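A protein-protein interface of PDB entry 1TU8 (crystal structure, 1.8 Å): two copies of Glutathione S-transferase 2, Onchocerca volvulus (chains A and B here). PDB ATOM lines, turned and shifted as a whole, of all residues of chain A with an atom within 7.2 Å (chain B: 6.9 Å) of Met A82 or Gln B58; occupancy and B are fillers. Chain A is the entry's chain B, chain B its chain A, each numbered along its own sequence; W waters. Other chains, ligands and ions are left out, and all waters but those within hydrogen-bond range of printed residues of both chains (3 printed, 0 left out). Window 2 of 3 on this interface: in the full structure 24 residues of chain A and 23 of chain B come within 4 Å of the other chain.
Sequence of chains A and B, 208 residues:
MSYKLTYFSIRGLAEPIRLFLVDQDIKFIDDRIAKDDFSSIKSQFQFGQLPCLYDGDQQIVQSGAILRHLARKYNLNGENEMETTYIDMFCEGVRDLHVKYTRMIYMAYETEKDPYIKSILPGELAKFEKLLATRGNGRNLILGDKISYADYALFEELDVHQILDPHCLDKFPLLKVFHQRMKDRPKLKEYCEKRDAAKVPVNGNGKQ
The backbone NH (N) of Leu B53 sits at hydrogen-bond distance from the backbone carbonyl oxygen (O) of Ile B60 (2.8 Å). The side-chain carboxylate (OD2) of Asp B55 is in hydrogen-bond range of a ring nitrogen (NE2) of His B69, 2.7 Å away. The backbone NH (N) of Met A82 lies close to the side-chain amide nitrogen (ND2) of Asn A80, at 3.2 Å. The side-chain hydroxyl of Thr A84 is in hydrogen-bond range of the backbone carbonyl oxygen of Asn A80 (3.1 Å). The backbone carbonyl oxygen (O) of Glu A81 lies within hydrogen-bond range of the side-chain hydroxyl (OG1) of Thr A85 (3.0 Å).
Of the 13 printed residues of chain B, 4 touch a printed residue of chain A. Along chain B the printed residues that touch a printed residue of chain A span positions 58 to 72. Of the 13 printed residues of chain A, 4 touch a printed residue of chain B. Hydrophobic or aromatic side chains of chain A that line the printed part of chain B: Met A82. Along chain A the printed residues that touch a printed residue of chain B span positions 81 to 85.
No position is printed for both chains. Of the 7 pairs that touch across the chains among the printed residues, none has its exchanged pair printed and touching as well.
Of chain B, only Gln B58 comes within 4 Å of Met A82. Printed residues of chain B within 4 Å of Thr A85: Ile B60 (3.7 Å), His B69 (3.6 Å) and Arg B72 (3.1 Å). Of the printed residues of chain A, Gln B58 touches Met A82. Of the printed residues of chain A, Arg B72 touches Glu A81 (2.9 Å), Thr A84 (3.5 Å) and Thr A85 (3.1 Å). The nearest residue of chain A that does not touch Gln B58 is Thr A85 (5.2 Å).
Water W3 lies within hydrogen-bond range of the side-chain amide nitrogen (NE2) of Gln B58 (2.5 Å), the side-chain hydroxyl (OG1) of Thr A85 (2.9 Å) and the backbone carbonyl oxygen (O) of Glu A81 (3.5 Å). Water W1 lies within hydrogen-bond range of the side-chain carboxylate (OD2) of Asp A88 and the guanidinium group (NH1) of Arg B72. Water W2 lies within hydrogen-bond range of OD2 of Asp A88 and NH2 of Arg B72.
A ring nitrogen (ND1) of His B69 lies within hydrogen-bond range of the side-chain carboxylate (OE1) of Glu A81, at 2.6 Å. The guanidinium group of Arg B72 lies within salt-bridge range of the side-chain carboxylate of Glu A81, at 2.9 Å. NH2 of Arg B72 lies within hydrogen-bond range of OG1 of Thr A85 (3.1 Å).
Gln B58 touches Met A82. CZ of Arg B72 touches CG2 of Thr A84 (3.5 Å). Thr A85 touches Ile B60 (CG2 to CG2, 3.7 Å). Thr A85 touches His B69.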
ATOM      1  N   GLY A  78       7.531  -7.877 -12.047  1.00  0.00           N
ATOM      2  CA  GLY A  78       8.277  -8.628 -13.043  1.00  0.00           C
ATOM      3  C   GLY A  78       9.790  -8.546 -12.852  1.00  0.00           C
ATOM      4  O   GLY A  78      10.298  -7.649 -12.169  1.00  0.00           O
ATOM      5  N   GLU A  79      10.509  -9.471 -13.489  1.00  0.00           N
ATOM      6  CA  GLU A  79      11.968  -9.572 -13.358  1.00  0.00           C
ATOM      7  C   GLU A  79      12.763  -8.883 -14.480  1.00  0.00           C
ATOM      8  O   GLU A  79      13.959  -8.626 -14.320  1.00  0.00           O
ATOM      9  CB  GLU A  79      12.382 -11.043 -13.272  1.00  0.00           C
ATOM     10  CG  GLU A  79      12.064 -11.681 -11.931  1.00  0.00           C
ATOM     11  CD  GLU A  79      12.562 -13.114 -11.823  1.00  0.00           C
ATOM     12  OE1 GLU A  79      12.139 -13.813 -10.877  1.00  0.00           O
ATOM     13  OE2 GLU A  79      13.368 -13.545 -12.677  1.00  0.00           O
ATOM     14  N   ASN A  80      12.111  -8.606 -15.607  1.00  0.00           N
ATOM     15  CA  ASN A  80      12.716  -7.833 -16.695  1.00  0.00           C
ATOM     16  C   ASN A  80      11.665  -6.971 -17.383  1.00  0.00           C
ATOM     17  O   ASN A  80      10.494  -7.043 -17.027  1.00  0.00           O
ATOM     18  CB  ASN A  80      13.417  -8.752 -17.705  1.00  0.00           C
ATOM     19  CG  ASN A  80      12.518  -9.875 -18.201  1.00  0.00           C
ATOM     20  OD1 ASN A  80      12.805 -11.057 -17.985  1.00  0.00           O
ATOM     21  ND2 ASN A  80      11.431  -9.516 -18.860  1.00  0.00           N
ATOM     22  N   GLU A  81      12.089  -6.161 -18.352  1.00  0.00           N
ATOM     23  CA  GLU A  81      11.217  -5.197 -19.037  1.00  0.00           C
ATOM     24  C   GLU A  81      10.001  -5.844 -19.665  1.00  0.00           C
ATOM     25  O   GLU A  81       8.909  -5.291 -19.600  1.00  0.00           O
ATOM     26  CB  GLU A  81      11.979  -4.456 -20.155  1.00  0.00           C
ATOM     27  CG  GLU A  81      11.101  -3.599 -21.083  1.00  0.00           C
ATOM     28  CD  GLU A  81      10.440  -2.463 -20.338  1.00  0.00           C
ATOM     29  OE1 GLU A  81       9.363  -2.027 -20.748  1.00  0.00           O
ATOM     30  OE2 GLU A  81      11.013  -2.001 -19.319  1.00  0.00           O
ATOM     31  N   MET A  82      10.212  -6.989 -20.310  1.00  0.00           N
ATOM     32  CA  MET A  82       9.143  -7.682 -21.014  1.00  0.00           C
ATOM     33  C   MET A  82       8.085  -8.200 -20.043  1.00  0.00           C
ATOM     34  O   MET A  82       6.903  -8.130 -20.333  1.00  0.00           O
ATOM     35  CB  MET A  82       9.692  -8.828 -21.879  1.00  0.00           C
ATOM     36  CG  MET A  82       9.958  -8.425 -23.317  1.00  0.00           C
ATOM     37  SD  MET A  82      11.260  -9.417 -24.098  1.00  0.00           S
ATOM     38  CE  MET A  82      10.650  -9.570 -25.789  1.00  0.00           C
ATOM     39  N   GLU A  83       8.515  -8.705 -18.889  1.00  0.00           N
ATOM     40  CA  GLU A  83       7.582  -9.182 -17.880  1.00  0.00           C
ATOM     41  C   GLU A  83       6.793  -8.000 -17.307  1.00  0.00           C
ATOM     42  O   GLU A  83       5.586  -8.098 -17.114  1.00  0.00           O
ATOM     43  CB  GLU A  83       8.311  -9.930 -16.762  1.00  0.00           C
ATOM     44  CG  GLU A  83       8.876 -11.275 -17.208  1.00  0.00           C
ATOM     45  CD  GLU A  83       9.286 -12.172 -16.055  1.00  0.00           C
ATOM     46  OE1 GLU A  83       9.629 -13.352 -16.319  1.00  0.00           O
ATOM     47  OE2 GLU A  83       9.276 -11.723 -14.892  1.00  0.00           O
ATOM     48  N   THR A  84       7.484  -6.891 -17.060  1.00  0.00           N
ATOM     49  CA  THR A  84       6.875  -5.667 -16.523  1.00  0.00           C
ATOM     50  C   THR A  84       5.789  -5.152 -17.466  1.00  0.00           C
ATOM     51  O   THR A  84       4.700  -4.750 -17.044  1.00  0.00           O
ATOM     52  CB  THR A  84       7.964  -4.586 -16.309  1.00  0.00           C
ATOM     53  OG1 THR A  84       8.893  -5.014 -15.299  1.00  0.00           O
ATOM     54  CG2 THR A  84       7.366  -3.263 -15.755  1.00  0.00           C
ATOM     55  N   THR A  85       6.095  -5.160 -18.753  1.00  0.00           N
ATOM     56  CA  THR A  85       5.144  -4.732 -19.768  1.00  0.00           C
ATOM     57  C   THR A  85       3.965  -5.682 -19.849  1.00  0.00           C
ATOM     58  O   THR A  85       2.826  -5.262 -19.983  1.00  0.00           O
ATOM     59  CB  THR A  85       5.831  -4.685 -21.132  1.00  0.00           C
ATOM     60  OG1 THR A  85       6.863  -3.702 -21.103  1.00  0.00           O
ATOM     61  CG2 THR A  85       4.876  -4.210 -22.211  1.00  0.00           C
ATOM     62  N   TYR A  86       4.256  -6.973 -19.774  1.00  0.00           N
ATOM     63  CA  TYR A  86       3.235  -7.992 -19.944  1.00  0.00           C
ATOM     64  C   TYR A  86       2.203  -7.936 -18.828  1.00  0.00           C
ATOM     65  O   TYR A  86       1.006  -7.969 -19.096  1.00  0.00           O
ATOM     66  CB  TYR A  86       3.868  -9.375 -19.957  1.00  0.00           C
ATOM     67  CG  TYR A  86       2.863 -10.493 -20.015  1.00  0.00           C
ATOM     68  CD1 TYR A  86       2.720 -11.376 -18.951  1.00  0.00           C
ATOM     69  CD2 TYR A  86       2.059 -10.675 -21.132  1.00  0.00           C
ATOM     70  CE1 TYR A  86       1.802 -12.411 -19.000  1.00  0.00           C
ATOM     71  CE2 TYR A  86       1.136 -11.713 -21.187  1.00  0.00           C
ATOM     72  CZ  TYR A  86       1.016 -12.578 -20.120  1.00  0.00           C
ATOM     73  OH  TYR A  86       0.100 -13.616 -20.163  1.00  0.00           O
ATOM     74  N   ILE A  87       2.661  -7.861 -17.580  1.00  0.00           N
ATOM     75  CA  ILE A  87       1.720  -7.836 -16.464  1.00  0.00           C
ATOM     76  C   ILE A  87       0.926  -6.545 -16.468  1.00  0.00           C
ATOM     77  O   ILE A  87      -0.219  -6.534 -16.051  1.00  0.00           O
ATOM     78  CB  ILE A  87       2.404  -8.099 -15.106  1.00  0.00           C
ATOM     79  CG1 ILE A  87       3.386  -6.982 -14.725  1.00  0.00           C
ATOM     80  CG2 ILE A  87       3.093  -9.466 -15.146  1.00  0.00           C
ATOM     81  CD1 ILE A  87       4.021  -7.197 -13.379  1.00  0.00           C
ATOM     82  N   ASP A  88       1.534  -5.463 -16.950  1.00  0.00           N
ATOM     83  CA  ASP A  88       0.844  -4.172 -17.083  1.00  0.00           C
ATOM     84  C   ASP A  88      -0.275  -4.289 -18.107  1.00  0.00           C
ATOM     85  O   ASP A  88      -1.429  -3.957 -17.842  1.00  0.00           O
ATOM     86  CB  ASP A  88       1.860  -3.107 -17.483  1.00  0.00           C
ATOM     87  CG  ASP A  88       1.307  -1.697 -17.462  1.00  0.00           C
ATOM     88  OD1 ASP A  88       0.104  -1.484 -17.191  1.00  0.00           O
ATOM     89  OD2 ASP A  88       2.060  -0.727 -17.691  1.00  0.00           O
ATOM     90  N   ARG A 135       2.381 -18.071 -20.143  1.00  0.00           N
ATOM     91  CA  ARG A 135       3.474 -18.358 -19.217  1.00  0.00           C
ATOM     92  C   ARG A 135       3.106 -19.509 -18.286  1.00  0.00           C
ATOM     93  O   ARG A 135       2.006 -19.536 -17.731  1.00  0.00           O
ATOM     94  CB  ARG A 135       3.842 -17.101 -18.423  1.00  0.00           C
ATOM     95  CG  ARG A 135       4.737 -16.135 -19.207  1.00  0.00           C
ATOM     96  CD  ARG A 135       4.558 -14.671 -18.836  1.00  0.00           C
ATOM     97  NE  ARG A 135       4.903 -13.764 -19.936  1.00  0.00           N
ATOM     98  CZ  ARG A 135       6.139 -13.387 -20.268  1.00  0.00           C
ATOM     99  NH1 ARG A 135       7.197 -13.836 -19.600  1.00  0.00           N
ATOM    100  NH2 ARG A 135       6.318 -12.555 -21.288  1.00  0.00           N
ATOM    101  N   LEU A 143       2.765 -14.862 -14.421  1.00  0.00           N
ATOM    102  CA  LEU A 143       4.155 -14.949 -14.889  1.00  0.00           C
ATOM    103  C   LEU A 143       4.753 -16.355 -14.767  1.00  0.00           C
ATOM    104  O   LEU A 143       5.915 -16.568 -15.132  1.00  0.00           O
ATOM    105  CB  LEU A 143       5.041 -13.941 -14.141  1.00  0.00           C
ATOM    106  CG  LEU A 143       4.853 -12.473 -14.549  1.00  0.00           C
ATOM    107  CD1 LEU A 143       5.769 -11.588 -13.726  1.00  0.00           C
ATOM    108  CD2 LEU A 143       5.097 -12.241 -16.028  1.00  0.00           C
ATOM    109  N   GLN B  46      -4.592  -9.084 -28.486  1.00  0.00           N
ATOM    110  CA  GLN B  46      -4.814  -9.854 -27.262  1.00  0.00           C
ATOM    111  C   GLN B  46      -6.173  -9.572 -26.596  1.00  0.00           C
ATOM    112  O   GLN B  46      -6.746 -10.456 -25.955  1.00  0.00           O
ATOM    113  CB  GLN B  46      -3.662  -9.631 -26.269  1.00  0.00           C
ATOM    114  CG  GLN B  46      -2.309 -10.254 -26.692  1.00  0.00           C
ATOM    115  CD  GLN B  46      -1.344  -9.260 -27.342  1.00  0.00           C
ATOM    116  OE1 GLN B  46      -0.131  -9.310 -27.107  1.00  0.00           O
ATOM    117  NE2 GLN B  46      -1.872  -8.375 -28.157  1.00  0.00           N
ATOM    118  N   CYS B  52      -2.114  -0.875 -30.838  1.00  0.00           N
ATOM    119  CA  CYS B  52      -1.094  -1.909 -30.696  1.00  0.00           C
ATOM    120  C   CYS B  52       0.243  -1.333 -31.110  1.00  0.00           C
ATOM    121  O   CYS B  52       0.349  -0.749 -32.182  1.00  0.00           O
ATOM    122  CB  CYS B  52      -1.403  -3.105 -31.585  1.00  0.00           C
ATOM    123  SG  CYS B  52      -0.266  -4.483 -31.340  1.00  0.00           S
ATOM    124  N   LEU B  53       1.263  -1.482 -30.262  1.00  0.00           N
ATOM    125  CA  LEU B  53       2.624  -1.158 -30.642  1.00  0.00           C
ATOM    126  C   LEU B  53       3.388  -2.446 -30.873  1.00  0.00           C
ATOM    127  O   LEU B  53       3.502  -3.267 -29.971  1.00  0.00           O
ATOM    128  CB  LEU B  53       3.312  -0.334 -29.556  1.00  0.00           C
ATOM    129  CG  LEU B  53       4.763   0.057 -29.867  1.00  0.00           C
ATOM    130  CD1 LEU B  53       4.822   1.162 -30.917  1.00  0.00           C
ATOM    131  CD2 LEU B  53       5.523   0.458 -28.607  1.00  0.00           C
ATOM    132  N   TYR B  54       3.893  -2.618 -32.091  1.00  0.00           N
ATOM    133  CA  TYR B  54       4.847  -3.658 -32.380  1.00  0.00           C
ATOM    134  C   TYR B  54       6.210  -3.037 -32.143  1.00  0.00           C
ATOM    135  O   TYR B  54       6.610  -2.119 -32.847  1.00  0.00           O
ATOM    136  CB  TYR B  54       4.710  -4.147 -33.824  1.00  0.00           C
ATOM    137  CG  TYR B  54       3.352  -4.714 -34.163  1.00  0.00           C
ATOM    138  CD1 TYR B  54       2.324  -3.893 -34.639  1.00  0.00           C
ATOM    139  CD2 TYR B  54       3.096  -6.075 -34.028  1.00  0.00           C
ATOM    140  CE1 TYR B  54       1.070  -4.424 -34.971  1.00  0.00           C
ATOM    141  CE2 TYR B  54       1.851  -6.607 -34.354  1.00  0.00           C
ATOM    142  CZ  TYR B  54       0.852  -5.780 -34.829  1.00  0.00           C
ATOM    143  OH  TYR B  54      -0.370  -6.312 -35.159  1.00  0.00           O
ATOM    144  N   ASP B  55       6.883  -3.510 -31.103  1.00  0.00           N
ATOM    145  CA  ASP B  55       8.229  -3.102 -30.768  1.00  0.00           C
ATOM    146  C   ASP B  55       9.146  -4.279 -31.090  1.00  0.00           C
ATOM    147  O   ASP B  55       9.276  -5.216 -30.303  1.00  0.00           O
ATOM    148  CB  ASP B  55       8.270  -2.727 -29.284  1.00  0.00           C
ATOM    149  CG  ASP B  55       9.639  -2.302 -28.817  1.00  0.00           C
ATOM    150  OD1 ASP B  55      10.634  -2.492 -29.565  1.00  0.00           O
ATOM    151  OD2 ASP B  55       9.806  -1.772 -27.690  1.00  0.00           O
ATOM    152  N   GLY B  56       9.797  -4.222 -32.250  1.00  0.00           N
ATOM    153  CA  GLY B  56      10.541  -5.360 -32.756  1.00  0.00           C
ATOM    154  C   GLY B  56       9.595  -6.541 -32.863  1.00  0.00           C
ATOM    155  O   GLY B  56       8.561  -6.445 -33.508  1.00  0.00           O
ATOM    156  N   ASP B  57       9.921  -7.625 -32.168  1.00  0.00           N
ATOM    157  CA  ASP B  57       9.118  -8.845 -32.195  1.00  0.00           C
ATOM    158  C   ASP B  57       7.999  -8.860 -31.143  1.00  0.00           C
ATOM    159  O   ASP B  57       7.166  -9.768 -31.153  1.00  0.00           O
ATOM    160  CB  ASP B  57      10.026 -10.069 -31.953  1.00  0.00           C
ATOM    161  CG  ASP B  57      10.633 -10.636 -33.238  1.00  0.00           C
ATOM    162  OD1 ASP B  57      11.797 -10.248 -33.625  1.00  0.00           O
ATOM    163  OD2 ASP B  57       9.975 -11.502 -33.931  1.00  0.00           O
ATOM    164  N   GLN B  58       7.973  -7.860 -30.258  1.00  0.00           N
ATOM    165  CA  GLN B  58       6.961  -7.756 -29.194  1.00  0.00           C
ATOM    166  C   GLN B  58       5.685  -7.115 -29.719  1.00  0.00           C
ATOM    167  O   GLN B  58       5.745  -6.124 -30.434  1.00  0.00           O
ATOM    168  CB  GLN B  58       7.462  -6.891 -28.036  1.00  0.00           C
ATOM    169  CG  GLN B  58       8.785  -7.288 -27.446  1.00  0.00           C
ATOM    170  CD  GLN B  58       9.310  -6.247 -26.472  1.00  0.00           C
ATOM    171  OE1 GLN B  58      10.401  -5.693 -26.668  1.00  0.00           O
ATOM    172  NE2 GLN B  58       8.536  -5.966 -25.426  1.00  0.00           N
ATOM    173  N   GLN B  59       4.539  -7.682 -29.359  1.00  0.00           N
ATOM    174  CA  GLN B  59       3.237  -7.111 -29.676  1.00  0.00           C
ATOM    175  C   GLN B  59       2.579  -6.643 -28.378  1.00  0.00           C
ATOM    176  O   GLN B  59       2.235  -7.454 -27.521  1.00  0.00           O
ATOM    177  CB  GLN B  59       2.344  -8.146 -30.365  1.00  0.00           C
ATOM    178  CG  GLN B  59       1.020  -7.566 -30.828  1.00  0.00           C
ATOM    179  CD  GLN B  59       0.026  -8.600 -31.312  1.00  0.00           C
ATOM    180  OE1 GLN B  59       0.207  -9.802 -31.107  1.00  0.00           O
ATOM    181  NE2 GLN B  59      -1.034  -8.132 -31.950  1.00  0.00           N
ATOM    182  N   ILE B  60       2.412  -5.331 -28.248  1.00  0.00           N
ATOM    183  CA  ILE B  60       1.964  -4.710 -27.008  1.00  0.00           C
ATOM    184  C   ILE B  60       0.689  -3.926 -27.261  1.00  0.00           C
ATOM    185  O   ILE B  60       0.709  -2.904 -27.945  1.00  0.00           O
ATOM    186  CB  ILE B  60       3.038  -3.753 -26.427  1.00  0.00           C
ATOM    187  CG1 ILE B  60       4.416  -4.428 -26.371  1.00  0.00           C
ATOM    188  CG2 ILE B  60       2.624  -3.286 -25.024  1.00  0.00           C
ATOM    189  CD1 ILE B  60       5.560  -3.465 -26.182  1.00  0.00           C
ATOM    190  N   HIS B  69       5.796   1.466 -21.119  1.00  0.00           N
ATOM    191  CA  HIS B  69       6.922   0.703 -21.672  1.00  0.00           C
ATOM    192  C   HIS B  69       7.897   1.629 -22.415  1.00  0.00           C
ATOM    193  O   HIS B  69       9.110   1.560 -22.202  1.00  0.00           O
ATOM    194  CB  HIS B  69       6.423  -0.458 -22.558  1.00  0.00           C
ATOM    195  CG  HIS B  69       7.446  -0.958 -23.532  1.00  0.00           C
ATOM    196  ND1 HIS B  69       8.707  -1.359 -23.145  1.00  0.00           N
ATOM    197  CD2 HIS B  69       7.399  -1.108 -24.875  1.00  0.00           C
ATOM    198  CE1 HIS B  69       9.398  -1.718 -24.212  1.00  0.00           C
ATOM    199  NE2 HIS B  69       8.626  -1.579 -25.274  1.00  0.00           N
ATOM    200  N   ARG B  72       9.893   3.737 -19.932  1.00  0.00           N
ATOM    201  CA  ARG B  72      11.001   2.999 -19.321  1.00  0.00           C
ATOM    202  C   ARG B  72      12.160   2.898 -20.297  1.00  0.00           C
ATOM    203  O   ARG B  72      13.312   3.141 -19.952  1.00  0.00           O
ATOM    204  CB  ARG B  72      10.575   1.589 -18.926  1.00  0.00           C
ATOM    205  CG  ARG B  72       9.782   1.526 -17.653  1.00  0.00           C
ATOM    206  CD  ARG B  72       9.575   0.114 -17.166  1.00  0.00           C
ATOM    207  NE  ARG B  72       8.766  -0.689 -18.077  1.00  0.00           N
ATOM    208  CZ  ARG B  72       7.434  -0.707 -18.095  1.00  0.00           C
ATOM    209  NH1 ARG B  72       6.729   0.027 -17.250  1.00  0.00           N
ATOM    210  NH2 ARG B  72       6.804  -1.487 -18.958  1.00  0.00           N
ATOM    211  N   LYS B  73      11.838   2.560 -21.534  1.00  0.00           N
ATOM    212  CA  LYS B  73      12.835   2.251 -22.541  1.00  0.00           C
ATOM    213  C   LYS B  73      13.669   3.475 -22.929  1.00  0.00           C
ATOM    214  O   LYS B  73      14.851   3.346 -23.219  1.00  0.00           O
ATOM    215  CB  LYS B  73      12.133   1.634 -23.758  1.00  0.00           C
ATOM    216  CG  LYS B  73      13.047   1.108 -24.813  1.00  0.00           C
ATOM    217  CD  LYS B  73      12.391  -0.052 -25.545  1.00  0.00           C
ATOM    218  CE  LYS B  73      13.212  -0.522 -26.732  1.00  0.00           C
ATOM    219  NZ  LYS B  73      12.347  -0.548 -27.937  1.00  0.00           N
HETATM  220  O   HOH W   1       4.174  -0.681 -15.960  1.00  0.00           O
HETATM  221  O   HOH W   2       4.043  -1.243 -19.577  1.00  0.00           O
HETATM  222  O   HOH W   3       8.588  -5.026 -23.064  1.00  0.00           O
